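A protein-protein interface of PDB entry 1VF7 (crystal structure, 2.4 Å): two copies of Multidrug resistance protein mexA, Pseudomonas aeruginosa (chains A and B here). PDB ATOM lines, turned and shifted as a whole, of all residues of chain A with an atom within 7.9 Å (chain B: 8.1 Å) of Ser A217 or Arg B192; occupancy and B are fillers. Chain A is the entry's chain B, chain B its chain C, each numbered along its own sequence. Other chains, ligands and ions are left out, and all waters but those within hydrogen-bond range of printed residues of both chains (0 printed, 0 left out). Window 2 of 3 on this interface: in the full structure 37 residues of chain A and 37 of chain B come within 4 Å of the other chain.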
ATOM      1  N   LEU A 211       4.327  -2.534 -22.818  1.00  0.00           N
ATOM      2  CA  LEU A 211       3.601  -2.917 -21.645  1.00  0.00           C
ATOM      3  C   LEU A 211       3.243  -1.712 -20.853  1.00  0.00           C
ATOM      4  O   LEU A 211       4.074  -0.818 -20.640  1.00  0.00           O
ATOM      5  CB  LEU A 211       4.405  -3.946 -20.799  1.00  0.00           C
ATOM      6  CG  LEU A 211       3.647  -4.690 -19.684  1.00  0.00           C
ATOM      7  CD1 LEU A 211       2.547  -5.614 -20.291  1.00  0.00           C
ATOM      8  CD2 LEU A 211       4.593  -5.480 -18.761  1.00  0.00           C
ATOM      9  N   LYS A 212       2.006  -1.708 -20.401  1.00  0.00           N
ATOM     10  CA  LYS A 212       1.568  -0.673 -19.549  1.00  0.00           C
ATOM     11  C   LYS A 212       1.176  -1.333 -18.254  1.00  0.00           C
ATOM     12  O   LYS A 212       0.489  -2.350 -18.244  1.00  0.00           O
ATOM     13  CB  LYS A 212       0.389   0.100 -20.206  1.00  0.00           C
ATOM     14  CG  LYS A 212      -0.488   0.972 -19.247  1.00  0.00           C
ATOM     15  CD  LYS A 212      -1.777   1.492 -19.940  1.00  0.00           C
ATOM     16  CE  LYS A 212      -1.455   2.528 -21.098  1.00  0.00           C
ATOM     17  NZ  LYS A 212      -2.568   3.570 -21.348  1.00  0.00           N
ATOM     18  N   LEU A 213       1.611  -0.712 -17.171  1.00  0.00           N
ATOM     19  CA  LEU A 213       1.532  -1.285 -15.866  1.00  0.00           C
ATOM     20  C   LEU A 213       0.245  -0.912 -15.195  1.00  0.00           C
ATOM     21  O   LEU A 213      -0.507  -0.105 -15.715  1.00  0.00           O
ATOM     22  CB  LEU A 213       2.730  -0.811 -15.037  1.00  0.00           C
ATOM     23  CG  LEU A 213       4.096  -1.223 -15.605  1.00  0.00           C
ATOM     24  CD1 LEU A 213       5.187  -0.826 -14.656  1.00  0.00           C
ATOM     25  CD2 LEU A 213       4.145  -2.728 -15.870  1.00  0.00           C
ATOM     26  N   GLU A 214       0.015  -1.489 -14.024  1.00  0.00           N
ATOM     27  CA  GLU A 214      -1.226  -1.343 -13.295  1.00  0.00           C
ATOM     28  C   GLU A 214      -1.580   0.113 -12.998  1.00  0.00           C
ATOM     29  O   GLU A 214      -2.756   0.488 -13.011  1.00  0.00           O
ATOM     30  CB  GLU A 214      -1.144  -2.130 -11.987  1.00  0.00           C
ATOM     31  CG  GLU A 214      -2.357  -1.956 -11.077  1.00  0.00           C
ATOM     32  CD  GLU A 214      -2.606  -3.171 -10.202  1.00  0.00           C
ATOM     33  OE1 GLU A 214      -2.213  -4.301 -10.614  1.00  0.00           O
ATOM     34  OE2 GLU A 214      -3.185  -3.000  -9.101  1.00  0.00           O
ATOM     35  N   ASP A 215      -0.555   0.913 -12.722  1.00  0.00           N
ATOM     36  CA  ASP A 215      -0.683   2.326 -12.372  1.00  0.00           C
ATOM     37  C   ASP A 215      -0.635   3.210 -13.637  1.00  0.00           C
ATOM     38  O   ASP A 215      -0.229   4.363 -13.578  1.00  0.00           O
ATOM     39  CB  ASP A 215       0.485   2.696 -11.432  1.00  0.00           C
ATOM     40  CG  ASP A 215       1.839   2.632 -12.141  1.00  0.00           C
ATOM     41  OD1 ASP A 215       1.929   2.013 -13.219  1.00  0.00           O
ATOM     42  OD2 ASP A 215       2.870   3.195 -11.743  1.00  0.00           O
ATOM     43  N   GLY A 216      -0.998   2.663 -14.788  1.00  0.00           N
ATOM     44  CA  GLY A 216      -0.925   3.414 -16.051  1.00  0.00           C
ATOM     45  C   GLY A 216       0.458   3.703 -16.646  1.00  0.00           C
ATOM     46  O   GLY A 216       0.557   4.138 -17.821  1.00  0.00           O
ATOM     47  N   SER A 217       1.526   3.458 -15.868  1.00  0.00           N
ATOM     48  CA  SER A 217       2.893   3.800 -16.327  1.00  0.00           C
ATOM     49  C   SER A 217       3.346   2.907 -17.454  1.00  0.00           C
ATOM     50  O   SER A 217       2.799   1.822 -17.688  1.00  0.00           O
ATOM     51  CB  SER A 217       3.942   3.851 -15.185  1.00  0.00           C
ATOM     52  OG  SER A 217       4.094   2.614 -14.479  1.00  0.00           O
ATOM     53  N   GLN A 218       4.330   3.405 -18.169  1.00  0.00           N
ATOM     54  CA  GLN A 218       4.858   2.732 -19.306  1.00  0.00           C
ATOM     55  C   GLN A 218       6.125   2.002 -18.900  1.00  0.00           C
ATOM     56  O   GLN A 218       7.078   2.624 -18.398  1.00  0.00           O
ATOM     57  CB  GLN A 218       5.206   3.730 -20.404  1.00  0.00           C
ATOM     58  CG  GLN A 218       4.115   3.913 -21.431  1.00  0.00           C
ATOM     59  CD  GLN A 218       3.827   2.648 -22.232  1.00  0.00           C
ATOM     60  OE1 GLN A 218       4.721   2.085 -22.884  1.00  0.00           O
ATOM     61  NE2 GLN A 218       2.574   2.213 -22.192  1.00  0.00           N
ATOM     62  N   TYR A 219       6.136   0.692 -19.146  1.00  0.00           N
ATOM     63  CA  TYR A 219       7.329  -0.078 -18.960  1.00  0.00           C
ATOM     64  C   TYR A 219       8.211   0.286 -20.111  1.00  0.00           C
ATOM     65  O   TYR A 219       7.760   0.244 -21.247  1.00  0.00           O
ATOM     66  CB  TYR A 219       7.015  -1.577 -18.978  1.00  0.00           C
ATOM     67  CG  TYR A 219       8.193  -2.464 -18.658  1.00  0.00           C
ATOM     68  CD1 TYR A 219       8.811  -2.433 -17.368  1.00  0.00           C
ATOM     69  CD2 TYR A 219       8.673  -3.364 -19.607  1.00  0.00           C
ATOM     70  CE1 TYR A 219       9.873  -3.248 -17.072  1.00  0.00           C
ATOM     71  CE2 TYR A 219       9.744  -4.205 -19.313  1.00  0.00           C
ATOM     72  CZ  TYR A 219      10.345  -4.147 -18.031  1.00  0.00           C
ATOM     73  OH  TYR A 219      11.417  -4.993 -17.738  1.00  0.00           O
ATOM     74  N   PRO A 220       9.459   0.639 -19.826  1.00  0.00           N
ATOM     75  CA  PRO A 220      10.381   1.079 -20.855  1.00  0.00           C
ATOM     76  C   PRO A 220      10.764   0.065 -21.893  1.00  0.00           C
ATOM     77  O   PRO A 220      11.408   0.449 -22.851  1.00  0.00           O
ATOM     78  CB  PRO A 220      11.651   1.451 -20.065  1.00  0.00           C
ATOM     79  CG  PRO A 220      11.228   1.630 -18.648  1.00  0.00           C
ATOM     80  CD  PRO A 220      10.055   0.725 -18.474  1.00  0.00           C
ATOM     81  N   GLU A 251      12.098  -5.376 -11.992  1.00  0.00           N
ATOM     82  CA  GLU A 251      11.020  -4.389 -11.821  1.00  0.00           C
ATOM     83  C   GLU A 251       9.680  -5.109 -11.842  1.00  0.00           C
ATOM     84  O   GLU A 251       8.800  -4.789 -11.061  1.00  0.00           O
ATOM     85  CB  GLU A 251      11.009  -3.305 -12.921  1.00  0.00           C
ATOM     86  CG  GLU A 251      12.197  -2.351 -12.973  1.00  0.00           C
ATOM     87  CD  GLU A 251      12.220  -1.503 -14.300  1.00  0.00           C
ATOM     88  OE1 GLU A 251      13.017  -1.813 -15.325  1.00  0.00           O
ATOM     89  OE2 GLU A 251      11.376  -0.566 -14.342  1.00  0.00           O
ATOM     90  N   VAL A 258      -1.645  -6.076 -15.960  1.00  0.00           N
ATOM     91  CA  VAL A 258      -0.942  -5.221 -16.898  1.00  0.00           C
ATOM     92  C   VAL A 258      -1.722  -5.217 -18.211  1.00  0.00           C
ATOM     93  O   VAL A 258      -2.747  -5.907 -18.330  1.00  0.00           O
ATOM     94  CB  VAL A 258       0.545  -5.745 -17.129  1.00  0.00           C
ATOM     95  CG1 VAL A 258       1.454  -5.393 -15.964  1.00  0.00           C
ATOM     96  CG2 VAL A 258       0.577  -7.262 -17.426  1.00  0.00           C
ATOM     97  N   HIS A 259      -1.218  -4.486 -19.200  1.00  0.00           N
ATOM     98  CA  HIS A 259      -1.798  -4.473 -20.538  1.00  0.00           C
ATOM     99  C   HIS A 259      -0.743  -4.475 -21.594  1.00  0.00           C
ATOM    100  O   HIS A 259       0.066  -3.532 -21.696  1.00  0.00           O
ATOM    101  CB  HIS A 259      -2.664  -3.211 -20.757  1.00  0.00           C
ATOM    102  CG  HIS A 259      -3.815  -3.104 -19.813  1.00  0.00           C
ATOM    103  ND1 HIS A 259      -5.076  -3.584 -20.120  1.00  0.00           N
ATOM    104  CD2 HIS A 259      -3.889  -2.622 -18.548  1.00  0.00           C
ATOM    105  CE1 HIS A 259      -5.882  -3.384 -19.090  1.00  0.00           C
ATOM    106  NE2 HIS A 259      -5.189  -2.803 -18.123  1.00  0.00           N
ATOM    107  N   GLN A 261       0.335  -3.763 -25.332  1.00  0.00           N
ATOM    108  CA  GLN A 261      -0.070  -2.713 -26.228  1.00  0.00           C
ATOM    109  C   GLN A 261       0.431  -3.060 -27.591  1.00  0.00           C
ATOM    110  O   GLN A 261       1.652  -3.143 -27.834  1.00  0.00           O
ATOM    111  CB  GLN A 261       0.496  -1.373 -25.806  1.00  0.00           C
ATOM    112  CG  GLN A 261       0.007  -0.879 -24.480  1.00  0.00           C
ATOM    113  CD  GLN A 261       0.956   0.153 -23.892  1.00  0.00           C
ATOM    114  OE1 GLN A 261       2.185   0.062 -24.061  1.00  0.00           O
ATOM    115  NE2 GLN A 261       0.390   1.148 -23.208  1.00  0.00           N
ATOM    116  N   THR B 185       3.583  -2.829  -7.483  1.00  0.00           N
ATOM    117  CA  THR B 185       3.731  -1.581  -8.227  1.00  0.00           C
ATOM    118  C   THR B 185       4.064  -0.431  -7.274  1.00  0.00           C
ATOM    119  O   THR B 185       4.787   0.502  -7.659  1.00  0.00           O
ATOM    120  CB  THR B 185       2.494  -1.264  -9.145  1.00  0.00           C
ATOM    121  OG1 THR B 185       1.338  -0.995  -8.336  1.00  0.00           O
ATOM    122  CG2 THR B 185       2.085  -2.504  -9.977  1.00  0.00           C
ATOM    123  N   ALA B 186       3.579  -0.517  -6.030  1.00  0.00           N
ATOM    124  CA  ALA B 186       4.032   0.408  -4.977  1.00  0.00           C
ATOM    125  C   ALA B 186       5.546   0.271  -4.756  1.00  0.00           C
ATOM    126  O   ALA B 186       6.238   1.262  -4.551  1.00  0.00           O
ATOM    127  CB  ALA B 186       3.276   0.193  -3.695  1.00  0.00           C
ATOM    128  N   LEU B 187       6.054  -0.961  -4.814  1.00  0.00           N
ATOM    129  CA  LEU B 187       7.475  -1.200  -4.606  1.00  0.00           C
ATOM    130  C   LEU B 187       8.252  -0.598  -5.763  1.00  0.00           C
ATOM    131  O   LEU B 187       9.332  -0.014  -5.577  1.00  0.00           O
ATOM    132  CB  LEU B 187       7.812  -2.704  -4.483  1.00  0.00           C
ATOM    133  CG  LEU B 187       9.329  -3.067  -4.617  1.00  0.00           C
ATOM    134  CD1 LEU B 187      10.183  -2.494  -3.504  1.00  0.00           C
ATOM    135  CD2 LEU B 187       9.621  -4.551  -4.756  1.00  0.00           C
ATOM    136  N   LEU B 188       7.713  -0.776  -6.964  1.00  0.00           N
ATOM    137  CA  LEU B 188       8.329  -0.229  -8.167  1.00  0.00           C
ATOM    138  C   LEU B 188       8.390   1.294  -8.057  1.00  0.00           C
ATOM    139  O   LEU B 188       9.419   1.901  -8.312  1.00  0.00           O
ATOM    140  CB  LEU B 188       7.553  -0.681  -9.397  1.00  0.00           C
ATOM    141  CG  LEU B 188       8.077  -0.310 -10.791  1.00  0.00           C
ATOM    142  CD1 LEU B 188       9.632  -0.401 -10.946  1.00  0.00           C
ATOM    143  CD2 LEU B 188       7.384  -1.214 -11.771  1.00  0.00           C
ATOM    144  N   ARG B 189       7.294   1.885  -7.600  1.00  0.00           N
ATOM    145  CA  ARG B 189       7.253   3.301  -7.345  1.00  0.00           C
ATOM    146  C   ARG B 189       8.356   3.764  -6.398  1.00  0.00           C
ATOM    147  O   ARG B 189       9.027   4.772  -6.660  1.00  0.00           O
ATOM    148  CB  ARG B 189       5.878   3.696  -6.826  1.00  0.00           C
ATOM    149  CG  ARG B 189       5.911   5.027  -6.067  1.00  0.00           C
ATOM    150  CD  ARG B 189       4.818   5.196  -4.998  1.00  0.00           C
ATOM    151  NE  ARG B 189       5.289   6.078  -3.943  1.00  0.00           N
ATOM    152  CZ  ARG B 189       4.936   5.981  -2.669  1.00  0.00           C
ATOM    153  NH1 ARG B 189       4.094   5.038  -2.258  1.00  0.00           N
ATOM    154  NH2 ARG B 189       5.442   6.831  -1.787  1.00  0.00           N
ATOM    155  N   LEU B 190       8.572   3.038  -5.306  1.00  0.00           N
ATOM    156  CA  LEU B 190       9.619   3.401  -4.345  1.00  0.00           C
ATOM    157  C   LEU B 190      10.983   3.209  -4.921  1.00  0.00           C
ATOM    158  O   LEU B 190      11.886   3.925  -4.583  1.00  0.00           O
ATOM    159  CB  LEU B 190       9.518   2.525  -3.105  1.00  0.00           C
ATOM    160  CG  LEU B 190       8.404   2.829  -2.111  1.00  0.00           C
ATOM    161  CD1 LEU B 190       8.159   1.593  -1.198  1.00  0.00           C
ATOM    162  CD2 LEU B 190       8.730   4.083  -1.282  1.00  0.00           C
ATOM    163  N   ARG B 191      11.148   2.187  -5.753  1.00  0.00           N
ATOM    164  CA  ARG B 191      12.441   1.912  -6.381  1.00  0.00           C
ATOM    165  C   ARG B 191      12.843   3.046  -7.343  1.00  0.00           C
ATOM    166  O   ARG B 191      14.032   3.394  -7.426  1.00  0.00           O
ATOM    167  CB  ARG B 191      12.431   0.590  -7.146  1.00  0.00           C
ATOM    168  CG  ARG B 191      12.587  -0.642  -6.295  1.00  0.00           C
ATOM    169  CD  ARG B 191      12.691  -1.927  -7.110  1.00  0.00           C
ATOM    170  NE  ARG B 191      13.997  -1.988  -7.743  1.00  0.00           N
ATOM    171  CZ  ARG B 191      14.386  -2.868  -8.662  1.00  0.00           C
ATOM    172  NH1 ARG B 191      13.572  -3.803  -9.104  1.00  0.00           N
ATOM    173  NH2 ARG B 191      15.613  -2.792  -9.159  1.00  0.00           N
ATOM    174  N   ARG B 192      11.852   3.572  -8.073  1.00  0.00           N
ATOM    175  CA  ARG B 192      12.016   4.763  -8.894  1.00  0.00           C
ATOM    176  C   ARG B 192      12.588   5.895  -8.030  1.00  0.00           C
ATOM    177  O   ARG B 192      13.635   6.468  -8.370  1.00  0.00           O
ATOM    178  CB  ARG B 192      10.656   5.264  -9.403  1.00  0.00           C
ATOM    179  CG  ARG B 192       9.925   4.495 -10.500  1.00  0.00           C
ATOM    180  CD  ARG B 192       8.529   5.185 -10.766  1.00  0.00           C
ATOM    181  NE  ARG B 192       7.487   4.386 -11.445  1.00  0.00           N
ATOM    182  CZ  ARG B 192       7.689   3.406 -12.347  1.00  0.00           C
ATOM    183  NH1 ARG B 192       8.930   3.054 -12.721  1.00  0.00           N
ATOM    184  NH2 ARG B 192       6.629   2.792 -12.890  1.00  0.00           N
ATOM    185  N   GLU B 193      11.886   6.203  -6.923  1.00  0.00           N
ATOM    186  CA  GLU B 193      12.257   7.296  -6.035  1.00  0.00           C
ATOM    187  C   GLU B 193      13.617   7.105  -5.433  1.00  0.00           C
ATOM    188  O   GLU B 193      14.185   8.020  -4.830  1.00  0.00           O
ATOM    189  CB  GLU B 193      11.293   7.438  -4.907  1.00  0.00           C
ATOM    190  CG  GLU B 193       9.875   7.653  -5.337  1.00  0.00           C
ATOM    191  CD  GLU B 193       9.025   7.773  -4.119  1.00  0.00           C
ATOM    192  OE1 GLU B 193       7.780   7.692  -4.214  1.00  0.00           O
ATOM    193  OE2 GLU B 193       9.644   7.930  -3.040  1.00  0.00           O
ATOM    194  N   LEU B 194      14.158   5.911  -5.589  1.00  0.00           N
ATOM    195  CA  LEU B 194      15.460   5.693  -5.063  1.00  0.00           C
ATOM    196  C   LEU B 194      16.460   6.165  -6.089  1.00  0.00           C
ATOM    197  O   LEU B 194      17.346   6.945  -5.751  1.00  0.00           O
ATOM    198  CB  LEU B 194      15.690   4.222  -4.631  1.00  0.00           C
ATOM    199  CG  LEU B 194      17.107   4.058  -4.046  1.00  0.00           C
ATOM    200  CD1 LEU B 194      17.228   4.675  -2.661  1.00  0.00           C
ATOM    201  CD2 LEU B 194      17.600   2.637  -4.075  1.00  0.00           C
ATOM    202  N   ALA B 195      16.329   5.696  -7.332  1.00  0.00           N
ATOM    203  CA  ALA B 195      17.270   6.088  -8.385  1.00  0.00           C
ATOM    204  C   ALA B 195      17.185   7.593  -8.691  1.00  0.00           C
ATOM    205  O   ALA B 195      18.210   8.208  -9.006  1.00  0.00           O
ATOM    206  CB  ALA B 195      17.104   5.234  -9.671  1.00  0.00           C
ATOM    207  N   SER B 196      15.971   8.149  -8.561  1.00  0.00           N
ATOM    208  CA  SER B 196      15.694   9.596  -8.719  1.00  0.00           C
ATOM    209  C   SER B 196      16.386  10.450  -7.653  1.00  0.00           C
ATOM    210  O   SER B 196      16.820  11.562  -7.924  1.00  0.00           O
ATOM    211  CB  SER B 196      14.187   9.887  -8.773  1.00  0.00           C
ATOM    212  OG  SER B 196      13.658  10.282  -7.519  1.00  0.00           O
ATOM    213  N   GLY B 197      16.521   9.915  -6.446  1.00  0.00           N
ATOM    214  CA  GLY B 197      17.191  10.626  -5.369  1.00  0.00           C
ATOM    215  C   GLY B 197      16.161  11.113  -4.394  1.00  0.00           C
ATOM    216  O   GLY B 197      16.504  11.576  -3.320  1.00  0.00           O
ATOM    217  N   GLN B 198      14.890  11.002  -4.756  1.00  0.00           N
ATOM    218  CA  GLN B 198      13.813  11.398  -3.841  1.00  0.00           C
ATOM    219  C   GLN B 198      13.846  10.602  -2.506  1.00  0.00           C
ATOM    220  O   GLN B 198      13.355  11.089  -1.481  1.00  0.00           O
ATOM    221  CB  GLN B 198      12.451  11.260  -4.507  1.00  0.00           C
ATOM    222  CG  GLN B 198      11.301  11.728  -3.633  1.00  0.00           C
ATOM    223  CD  GLN B 198       9.936  11.586  -4.323  1.00  0.00           C
ATOM    224  OE1 GLN B 198       9.882  11.210  -5.508  1.00  0.00           O
ATOM    225  NE2 GLN B 198       8.835  11.890  -3.596  1.00  0.00           N
ATOM    226  N   LEU B 199      14.403   9.380  -2.537  1.00  0.00           N
ATOM    227  CA  LEU B 199      14.675   8.627  -1.316  1.00  0.00           C
ATOM    228  C   LEU B 199      16.169   8.658  -1.002  1.00  0.00           C
ATOM    229  O   LEU B 199      17.017   8.518  -1.886  1.00  0.00           O
ATOM    230  CB  LEU B 199      14.140   7.182  -1.395  1.00  0.00           C
ATOM    231  CG  LEU B 199      12.625   6.970  -1.391  1.00  0.00           C
ATOM    232  CD1 LEU B 199      12.277   5.497  -1.522  1.00  0.00           C
ATOM    233  CD2 LEU B 199      11.993   7.544  -0.163  1.00  0.00           C
ATOM    234  N   PHE B 227      15.521  -3.503  -1.247  1.00  0.00           N
ATOM    235  CA  PHE B 227      14.450  -3.537  -2.245  1.00  0.00           C
ATOM    236  C   PHE B 227      14.325  -4.846  -2.977  1.00  0.00           C
ATOM    237  O   PHE B 227      13.345  -5.094  -3.671  1.00  0.00           O
ATOM    238  CB  PHE B 227      14.558  -2.371  -3.224  1.00  0.00           C
ATOM    239  CG  PHE B 227      14.094  -1.080  -2.649  1.00  0.00           C
ATOM    240  CD1 PHE B 227      14.970  -0.020  -2.488  1.00  0.00           C
ATOM    241  CD2 PHE B 227      12.791  -0.926  -2.242  1.00  0.00           C
ATOM    242  CE1 PHE B 227      14.545   1.168  -1.922  1.00  0.00           C
ATOM    243  CE2 PHE B 227      12.349   0.273  -1.665  1.00  0.00           C
ATOM    244  CZ  PHE B 227      13.221   1.312  -1.499  1.00  0.00           C
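Among the printed residues, merely in contact across the chains: Glu A251 with Arg B191, Leu A213 with Leu B188, Glu A251 with Leu B188 and Glu A214 with Thr B185.
OD1 of Asp A215 sits at hydrogen-bond distance from OG of Ser A217 (2.6 Å).
No position is printed for both chains.
Of the 6 pairs that touch across the chains among the printed residues, none has its exchanged pair printed and touching as well.
Printed residues of chain A within 4 Å of Arg B191: Glu A251.
Of the printed residues of chain B, Glu A214 touches Thr B185.
Printed residues of chain A within 4 Å of Leu B188: Leu A213 (3.6 Å) and Glu A251 (3.8 Å).
Of the printed residues of chain A, Thr B185 touches Glu A214.
Leu B187 touches none of the printed residues of chain A.
The nearest residue of chain A that does not touch Arg B192 is Leu A213 (4.3 Å).
The guanidinium group (NH2) of Arg B192 lies within salt-bridge range of the side-chain carboxylate (OD2) of Asp A215.
The side-chain hydroxyl of Ser A217 is in hydrogen-bond range of the guanidinium group of Arg B192 (3.0 Å).
Hydrophobic or aromatic side chains of chain A that line the printed part of chain B: Leu A213.
Hydrophobic or aromatic side chains of chain B that line the printed part of chain A: Leu B188.
Among the printed residues, 6 pairs touch across the chains.
Among the printed residues, Asp or Glu carboxylates within 4 Å of a Lys or Arg side-chain nitrogen of the other chain: Asp A215 with Arg B192 (3.95 Å).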
